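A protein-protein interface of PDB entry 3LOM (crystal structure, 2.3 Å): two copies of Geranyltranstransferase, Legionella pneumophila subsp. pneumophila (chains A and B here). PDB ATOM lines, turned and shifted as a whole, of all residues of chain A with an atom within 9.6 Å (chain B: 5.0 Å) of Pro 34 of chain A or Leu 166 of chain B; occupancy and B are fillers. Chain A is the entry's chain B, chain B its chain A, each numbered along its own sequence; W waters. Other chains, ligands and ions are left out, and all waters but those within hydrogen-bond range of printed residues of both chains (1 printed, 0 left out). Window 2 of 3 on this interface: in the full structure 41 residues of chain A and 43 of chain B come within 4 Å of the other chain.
OG of Ser 158 of chain B lies within hydrogen-bond range of O of Ile 32 of chain A (2.7 Å). N of Ala 35 of chain A sits at hydrogen-bond distance from OG of Ser 162 of chain B (3.4 Å).
Hydrophobic or aromatic side chains of chain B within 4 Å of the printed part of chain A: Ile 157, Leu 166 and Leu 187. Of the 14 printed residues of chain A, 7 touch a printed residue of chain B. Hydrophobic or aromatic side chains of chain A that line the printed part of chain B: Ile 31, Ile 33, Pro 34, Ala 35, Ile 38 and Leu 118. Among the printed residues, no Asp or Glu carboxylate lies within 4 Å of a Lys or Arg side-chain nitrogen of the other chain.
Water W1 lies within hydrogen-bond range of OG1 of Thr 115 of chain A (2.7 Å) and OG of Ser 165 of chain B (2.7 Å).
The side-chain hydroxyl (OG) of Ser 162 of chain B lies within hydrogen-bond range of the backbone carbonyl oxygen (O) of Ile 157 of chain B (2.5 Å). O of Ser 165 of chain B sits at hydrogen-bond distance from OG of Ser 169 of chain B. The backbone carbonyl oxygen of Ile 31 of chain A lies within hydrogen-bond range of the guanidinium group of Arg 39 of chain A (2.5 Å).
Ile 31 of chain A touches Ile 157 of chain B. Ile 31 of chain A touches Ser 158 of chain B. Ile 157 of chain B touches Pro 34 of chain A (O to CD, 3.5 Å). Pro 34 of chain A touches Leu 166 of chain B (O to CD1, 3.8 Å). CD1 of Leu 187 of chain B touches CB of Pro 34 of chain A, at 3.7 Å. Ser 165 of chain B touches Ala 35 of chain A. Leu 166 of chain B touches Ala 35 of chain A. CD1 of Ile 38 of chain A touches CB of Ser 165 of chain B, at 3.7 Å. CD2 of Leu 118 of chain A touches CG of Gln 164 of chain B, 3.9 Å away. Leu 118 of chain A touches Ser 165 of chain B.
No position is printed for both chains. Of the 16 pairs that touch across the chains among the printed residues, none has its exchanged pair printed and touching as well.
Of the printed residues of chain B, Pro 34 of chain A touches Ile 157, Ser 162, Leu 166 and Leu 187. Of chain A, only Pro 34 and Ala 35 come within 4 Å of Leu 166 of chain B. No residue of chain A comes within 4 Å of Ser 169 of chain B. No residue of chain A comes within 4 Å of Glu 170 of chain B. Printed residues of chain A within 4 Å of Ser 158 of chain B: Ile 31 (3.5 Å) and Ile 32 (2.7 Å). Of the printed residues of chain A, Leu 187 of chain B touches Pro 34 (3.7 Å). Of the printed residues of chain B, Ile 31 of chain A touches Ile 157 (3.8 Å) and Ser 158 (3.5 Å). Printed residues of chain B within 4 Å of Leu 118 of chain A: Gln 164 (3.9 Å) and Ser 165 (3.6 Å). Ala 114 of chain A touches none of the printed residues of chain B. Ser 40 of chain A touches none of the printed residues of chain B.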
ATOM      1  N   LEU A  28      39.057  22.635  33.533  1.00  0.00           N
ATOM      2  CA  LEU A  28      37.843  21.929  33.119  1.00  0.00           C
ATOM      3  C   LEU A  28      36.814  21.832  34.261  1.00  0.00           C
ATOM      4  O   LEU A  28      35.629  22.118  34.057  1.00  0.00           O
ATOM      5  CB  LEU A  28      38.198  20.529  32.606  1.00  0.00           C
ATOM      6  CG  LEU A  28      37.653  20.050  31.256  1.00  0.00           C
ATOM      7  CD1 LEU A  28      37.824  18.547  31.137  1.00  0.00           C
ATOM      8  CD2 LEU A  28      36.197  20.430  31.025  1.00  0.00           C
ATOM      9  N   ILE A  31      34.654  24.992  35.044  1.00  0.00           N
ATOM     10  CA  ILE A  31      33.671  25.468  34.058  1.00  0.00           C
ATOM     11  C   ILE A  31      32.307  24.838  34.289  1.00  0.00           C
ATOM     12  O   ILE A  31      32.201  23.631  34.487  1.00  0.00           O
ATOM     13  CB  ILE A  31      34.106  25.175  32.575  1.00  0.00           C
ATOM     14  CG1 ILE A  31      35.556  25.600  32.303  1.00  0.00           C
ATOM     15  CG2 ILE A  31      33.126  25.815  31.557  1.00  0.00           C
ATOM     16  CD1 ILE A  31      35.830  27.112  32.375  1.00  0.00           C
ATOM     17  N   ILE A  32      31.263  25.657  34.254  1.00  0.00           N
ATOM     18  CA  ILE A  32      29.896  25.157  34.299  1.00  0.00           C
ATOM     19  C   ILE A  32      29.539  24.525  32.954  1.00  0.00           C
ATOM     20  O   ILE A  32      29.521  25.209  31.930  1.00  0.00           O
ATOM     21  CB  ILE A  32      28.899  26.287  34.636  1.00  0.00           C
ATOM     22  CG1 ILE A  32      29.269  26.969  35.973  1.00  0.00           C
ATOM     23  CG2 ILE A  32      27.452  25.770  34.610  1.00  0.00           C
ATOM     24  CD1 ILE A  32      29.357  26.029  37.198  1.00  0.00           C
ATOM     25  N   ILE A  33      29.293  23.214  32.956  1.00  0.00           N
ATOM     26  CA  ILE A  33      28.921  22.492  31.737  1.00  0.00           C
ATOM     27  C   ILE A  33      27.607  21.740  31.959  1.00  0.00           C
ATOM     28  O   ILE A  33      27.597  20.664  32.546  1.00  0.00           O
ATOM     29  CB  ILE A  33      30.041  21.530  31.236  1.00  0.00           C
ATOM     30  CG1 ILE A  33      31.394  22.243  31.147  1.00  0.00           C
ATOM     31  CG2 ILE A  33      29.693  20.971  29.868  1.00  0.00           C
ATOM     32  CD1 ILE A  33      32.581  21.312  30.920  1.00  0.00           C
ATOM     33  N   PRO A  34      26.488  22.315  31.490  1.00  0.00           N
ATOM     34  CA  PRO A  34      25.175  21.716  31.733  1.00  0.00           C
ATOM     35  C   PRO A  34      24.959  20.337  31.103  1.00  0.00           C
ATOM     36  O   PRO A  34      24.128  19.565  31.600  1.00  0.00           O
ATOM     37  CB  PRO A  34      24.207  22.756  31.153  1.00  0.00           C
ATOM     38  CG  PRO A  34      24.919  24.058  31.368  1.00  0.00           C
ATOM     39  CD  PRO A  34      26.372  23.712  31.033  1.00  0.00           C
ATOM     40  N   ALA A  35      25.707  20.035  30.042  1.00  0.00           N
ATOM     41  CA  ALA A  35      25.646  18.736  29.389  1.00  0.00           C
ATOM     42  C   ALA A  35      26.837  17.890  29.819  1.00  0.00           C
ATOM     43  O   ALA A  35      27.973  18.180  29.431  1.00  0.00           O
ATOM     44  CB  ALA A  35      25.617  18.892  27.876  1.00  0.00           C
ATOM     45  N   PRO A  36      26.583  16.843  30.634  1.00  0.00           N
ATOM     46  CA  PRO A  36      27.642  15.945  31.103  1.00  0.00           C
ATOM     47  C   PRO A  36      28.406  15.219  29.988  1.00  0.00           C
ATOM     48  O   PRO A  36      29.603  14.965  30.144  1.00  0.00           O
ATOM     49  CB  PRO A  36      26.899  14.945  31.997  1.00  0.00           C
ATOM     50  CG  PRO A  36      25.437  15.190  31.771  1.00  0.00           C
ATOM     51  CD  PRO A  36      25.307  16.596  31.333  1.00  0.00           C
ATOM     52  N   GLN A  37      27.737  14.898  28.882  1.00  0.00           N
ATOM     53  CA  GLN A  37      28.422  14.331  27.705  1.00  0.00           C
ATOM     54  C   GLN A  37      29.507  15.243  27.123  1.00  0.00           C
ATOM     55  O   GLN A  37      30.568  14.759  26.718  1.00  0.00           O
ATOM     56  CB  GLN A  37      27.423  13.964  26.616  1.00  0.00           C
ATOM     57  CG  GLN A  37      26.904  12.556  26.732  1.00  0.00           C
ATOM     58  CD  GLN A  37      27.797  11.545  26.048  1.00  0.00           C
ATOM     59  OE1 GLN A  37      28.400  10.698  26.711  1.00  0.00           O
ATOM     60  NE2 GLN A  37      27.891  11.625  24.714  1.00  0.00           N
ATOM     61  N   ILE A  38      29.250  16.553  27.100  1.00  0.00           N
ATOM     62  CA  ILE A  38      30.254  17.527  26.644  1.00  0.00           C
ATOM     63  C   ILE A  38      31.483  17.517  27.560  1.00  0.00           C
ATOM     64  O   ILE A  38      32.615  17.437  27.077  1.00  0.00           O
ATOM     65  CB  ILE A  38      29.670  18.968  26.515  1.00  0.00           C
ATOM     66  CG1 ILE A  38      28.563  19.037  25.454  1.00  0.00           C
ATOM     67  CG2 ILE A  38      30.768  19.983  26.235  1.00  0.00           C
ATOM     68  CD1 ILE A  38      28.935  18.477  24.067  1.00  0.00           C
ATOM     69  N   ARG A  39      31.242  17.566  28.872  1.00  0.00           N
ATOM     70  CA  ARG A  39      32.300  17.511  29.892  1.00  0.00           C
ATOM     71  C   ARG A  39      33.142  16.243  29.773  1.00  0.00           C
ATOM     72  O   ARG A  39      34.369  16.298  29.815  1.00  0.00           O
ATOM     73  CB  ARG A  39      31.699  17.619  31.305  1.00  0.00           C
ATOM     74  CG  ARG A  39      32.723  17.459  32.448  1.00  0.00           C
ATOM     75  CD  ARG A  39      32.107  17.647  33.845  1.00  0.00           C
ATOM     76  NE  ARG A  39      31.535  18.977  34.050  1.00  0.00           N
ATOM     77  CZ  ARG A  39      32.243  20.081  34.295  1.00  0.00           C
ATOM     78  NH1 ARG A  39      31.617  21.231  34.461  1.00  0.00           N
ATOM     79  NH2 ARG A  39      33.570  20.045  34.370  1.00  0.00           N
ATOM     80  N   SER A  40      32.468  15.108  29.612  1.00  0.00           N
ATOM     81  CA  SER A  40      33.135  13.818  29.480  1.00  0.00           C
ATOM     82  C   SER A  40      33.927  13.706  28.177  1.00  0.00           C
ATOM     83  O   SER A  40      35.090  13.291  28.184  1.00  0.00           O
ATOM     84  CB  SER A  40      32.118  12.676  29.595  1.00  0.00           C
ATOM     85  OG  SER A  40      32.777  11.422  29.710  1.00  0.00           O
ATOM     86  N   ALA A 114      28.031  13.831  16.547  1.00  0.00           N
ATOM     87  CA  ALA A 114      27.478  15.076  17.078  1.00  0.00           C
ATOM     88  C   ALA A 114      28.293  15.607  18.258  1.00  0.00           C
ATOM     89  O   ALA A 114      28.640  16.786  18.297  1.00  0.00           O
ATOM     90  CB  ALA A 114      26.018  14.862  17.494  1.00  0.00           C
ATOM     91  N   THR A 115      28.602  14.715  19.201  1.00  0.00           N
ATOM     92  CA  THR A 115      29.378  15.042  20.392  1.00  0.00           C
ATOM     93  C   THR A 115      30.784  15.490  20.018  1.00  0.00           C
ATOM     94  O   THR A 115      31.256  16.533  20.486  1.00  0.00           O
ATOM     95  CB  THR A 115      29.395  13.846  21.383  1.00  0.00           C
ATOM     96  OG1 THR A 115      28.054  13.604  21.834  1.00  0.00           O
ATOM     97  CG2 THR A 115      30.260  14.133  22.581  1.00  0.00           C
ATOM     98  N   LEU A 118      30.325  19.056  18.399  1.00  0.00           N
ATOM     99  CA  LEU A 118      30.014  20.012  19.466  1.00  0.00           C
ATOM    100  C   LEU A 118      31.160  20.268  20.445  1.00  0.00           C
ATOM    101  O   LEU A 118      31.413  21.416  20.821  1.00  0.00           O
ATOM    102  CB  LEU A 118      28.742  19.595  20.217  1.00  0.00           C
ATOM    103  CG  LEU A 118      27.451  19.738  19.405  1.00  0.00           C
ATOM    104  CD1 LEU A 118      26.308  19.011  20.058  1.00  0.00           C
ATOM    105  CD2 LEU A 118      27.074  21.203  19.106  1.00  0.00           C
ATOM    106  N   ILE B 157      30.492  26.080  25.861  1.00  0.00           N
ATOM    107  CA  ILE B 157      30.012  24.883  26.558  1.00  0.00           C
ATOM    108  C   ILE B 157      29.092  25.165  27.749  1.00  0.00           C
ATOM    109  O   ILE B 157      28.330  24.293  28.162  1.00  0.00           O
ATOM    110  CB  ILE B 157      31.177  23.953  26.987  1.00  0.00           C
ATOM    111  CG1 ILE B 157      32.123  24.653  27.972  1.00  0.00           C
ATOM    112  CG2 ILE B 157      31.930  23.463  25.763  1.00  0.00           C
ATOM    113  CD1 ILE B 157      33.403  23.840  28.295  1.00  0.00           C
ATOM    114  N   SER B 158      29.159  26.389  28.280  1.00  0.00           N
ATOM    115  CA  SER B 158      28.256  26.821  29.342  1.00  0.00           C
ATOM    116  C   SER B 158      26.928  27.299  28.773  1.00  0.00           C
ATOM    117  O   SER B 158      26.007  27.616  29.523  1.00  0.00           O
ATOM    118  CB  SER B 158      28.895  27.930  30.188  1.00  0.00           C
ATOM    119  OG  SER B 158      30.176  27.544  30.671  1.00  0.00           O
ATOM    120  N   SER B 162      26.251  23.126  24.979  1.00  0.00           N
ATOM    121  CA  SER B 162      25.509  22.227  25.875  1.00  0.00           C
ATOM    122  C   SER B 162      24.034  22.225  25.505  1.00  0.00           C
ATOM    123  O   SER B 162      23.391  21.172  25.506  1.00  0.00           O
ATOM    124  CB  SER B 162      25.690  22.609  27.343  1.00  0.00           C
ATOM    125  OG  SER B 162      26.966  22.201  27.811  1.00  0.00           O
ATOM    126  N   GLY B 163      23.517  23.403  25.157  1.00  0.00           N
ATOM    127  CA  GLY B 163      22.139  23.532  24.676  1.00  0.00           C
ATOM    128  C   GLY B 163      21.796  22.625  23.508  1.00  0.00           C
ATOM    129  O   GLY B 163      20.752  21.986  23.516  1.00  0.00           O
ATOM    130  N   GLN B 164      22.683  22.557  22.513  1.00  0.00           N
ATOM    131  CA  GLN B 164      22.438  21.726  21.333  1.00  0.00           C
ATOM    132  C   GLN B 164      22.651  20.234  21.615  1.00  0.00           C
ATOM    133  O   GLN B 164      21.867  19.398  21.162  1.00  0.00           O
ATOM    134  CB  GLN B 164      23.264  22.215  20.126  1.00  0.00           C
ATOM    135  CG  GLN B 164      23.194  21.332  18.837  1.00  0.00           C
ATOM    136  CD  GLN B 164      21.783  21.157  18.240  1.00  0.00           C
ATOM    137  OE1 GLN B 164      20.806  21.738  18.706  1.00  0.00           O
ATOM    138  NE2 GLN B 164      21.691  20.349  17.190  1.00  0.00           N
ATOM    139  N   SER B 165      23.699  19.916  22.374  1.00  0.00           N
ATOM    140  CA  SER B 165      23.954  18.544  22.841  1.00  0.00           C
ATOM    141  C   SER B 165      22.768  17.957  23.608  1.00  0.00           C
ATOM    142  O   SER B 165      22.360  16.818  23.353  1.00  0.00           O
ATOM    143  CB  SER B 165      25.220  18.496  23.705  1.00  0.00           C
ATOM    144  OG  SER B 165      25.413  17.208  24.273  1.00  0.00           O
ATOM    145  N   LEU B 166      22.201  18.747  24.519  1.00  0.00           N
ATOM    146  CA  LEU B 166      21.043  18.303  25.302  1.00  0.00           C
ATOM    147  C   LEU B 166      19.765  18.301  24.470  1.00  0.00           C
ATOM    148  O   LEU B 166      18.869  17.490  24.716  1.00  0.00           O
ATOM    149  CB  LEU B 166      20.860  19.143  26.574  1.00  0.00           C
ATOM    150  CG  LEU B 166      21.859  18.928  27.715  1.00  0.00           C
ATOM    151  CD1 LEU B 166      21.782  20.066  28.710  1.00  0.00           C
ATOM    152  CD2 LEU B 166      21.653  17.591  28.417  1.00  0.00           C
ATOM    153  N   ASP B 167      19.688  19.198  23.485  1.00  0.00           N
ATOM    154  CA  ASP B 167      18.571  19.212  22.539  1.00  0.00           C
ATOM    155  C   ASP B 167      18.522  17.904  21.738  1.00  0.00           C
ATOM    156  O   ASP B 167      17.453  17.375  21.474  1.00  0.00           O
ATOM    157  CB  ASP B 167      18.679  20.414  21.595  1.00  0.00           C
ATOM    158  CG  ASP B 167      17.442  20.610  20.736  1.00  0.00           C
ATOM    159  OD1 ASP B 167      16.692  21.569  20.990  1.00  0.00           O
ATOM    160  OD2 ASP B 167      17.222  19.823  19.795  1.00  0.00           O
ATOM    161  N   LEU B 168      19.685  17.394  21.362  1.00  0.00           N
ATOM    162  CA  LEU B 168      19.759  16.159  20.604  1.00  0.00           C
ATOM    163  C   LEU B 168      19.557  14.913  21.464  1.00  0.00           C
ATOM    164  O   LEU B 168      18.798  14.025  21.085  1.00  0.00           O
ATOM    165  CB  LEU B 168      21.083  16.083  19.847  1.00  0.00           C
ATOM    166  CG  LEU B 168      21.234  17.100  18.716  1.00  0.00           C
ATOM    167  CD1 LEU B 168      22.640  17.038  18.174  1.00  0.00           C
ATOM    168  CD2 LEU B 168      20.191  16.894  17.602  1.00  0.00           C
ATOM    169  N   SER B 169      20.221  14.849  22.616  1.00  0.00           N
ATOM    170  CA  SER B 169      20.170  13.647  23.456  1.00  0.00           C
ATOM    171  C   SER B 169      18.887  13.492  24.276  1.00  0.00           C
ATOM    172  O   SER B 169      18.338  12.389  24.351  1.00  0.00           O
ATOM    173  CB  SER B 169      21.409  13.535  24.353  1.00  0.00           C
ATOM    174  OG  SER B 169      21.476  14.602  25.285  1.00  0.00           O
ATOM    175  N   GLU B 170      18.400  14.582  24.873  1.00  0.00           N
ATOM    176  CA  GLU B 170      17.256  14.488  25.802  1.00  0.00           C
ATOM    177  C   GLU B 170      15.880  14.570  25.158  1.00  0.00           C
ATOM    178  O   GLU B 170      14.961  13.877  25.596  1.00  0.00           O
ATOM    179  CB  GLU B 170      17.340  15.518  26.939  1.00  0.00           C
ATOM    180  CG  GLU B 170      18.647  15.531  27.700  1.00  0.00           C
ATOM    181  CD  GLU B 170      19.129  14.144  28.079  1.00  0.00           C
ATOM    182  OE1 GLU B 170      20.222  13.749  27.613  1.00  0.00           O
ATOM    183  OE2 GLU B 170      18.416  13.448  28.835  1.00  0.00           O
ATOM    184  N   LEU B 171      15.732  15.408  24.131  1.00  0.00           N
ATOM    185  CA  LEU B 171      14.419  15.656  23.508  1.00  0.00           C
ATOM    186  C   LEU B 171      13.852  14.451  22.757  1.00  0.00           C
ATOM    187  O   LEU B 171      12.656  14.413  22.456  1.00  0.00           O
ATOM    188  CB  LEU B 171      14.459  16.886  22.593  1.00  0.00           C
ATOM    189  CG  LEU B 171      13.910  18.236  23.080  1.00  0.00           C
ATOM    190  CD1 LEU B 171      14.382  18.609  24.479  1.00  0.00           C
ATOM    191  CD2 LEU B 171      14.259  19.341  22.090  1.00  0.00           C
ATOM    192  N   ILE B 184      16.966  23.859  28.250  1.00  0.00           N
ATOM    193  CA  ILE B 184      17.594  23.466  26.990  1.00  0.00           C
ATOM    194  C   ILE B 184      17.553  24.584  25.932  1.00  0.00           C
ATOM    195  O   ILE B 184      18.587  24.912  25.337  1.00  0.00           O
ATOM    196  CB  ILE B 184      16.990  22.133  26.462  1.00  0.00           C
ATOM    197  CG1 ILE B 184      17.512  20.960  27.303  1.00  0.00           C
ATOM    198  CG2 ILE B 184      17.344  21.911  24.999  1.00  0.00           C
ATOM    199  CD1 ILE B 184      16.599  19.747  27.343  1.00  0.00           C
ATOM    200  N   LEU B 187      19.731  27.592  26.888  1.00  0.00           N
ATOM    201  CA  LEU B 187      21.143  27.349  26.621  1.00  0.00           C
ATOM    202  C   LEU B 187      21.440  27.389  25.120  1.00  0.00           C
ATOM    203  O   LEU B 187      22.436  27.973  24.712  1.00  0.00           O
ATOM    204  CB  LEU B 187      21.606  26.027  27.237  1.00  0.00           C
ATOM    205  CG  LEU B 187      21.548  25.871  28.756  1.00  0.00           C
ATOM    206  CD1 LEU B 187      21.572  24.393  29.110  1.00  0.00           C
ATOM    207  CD2 LEU B 187      22.666  26.635  29.453  1.00  0.00           C
HETATM  208  O   HOH W   1      26.459  15.710  22.233  1.00  0.00           O
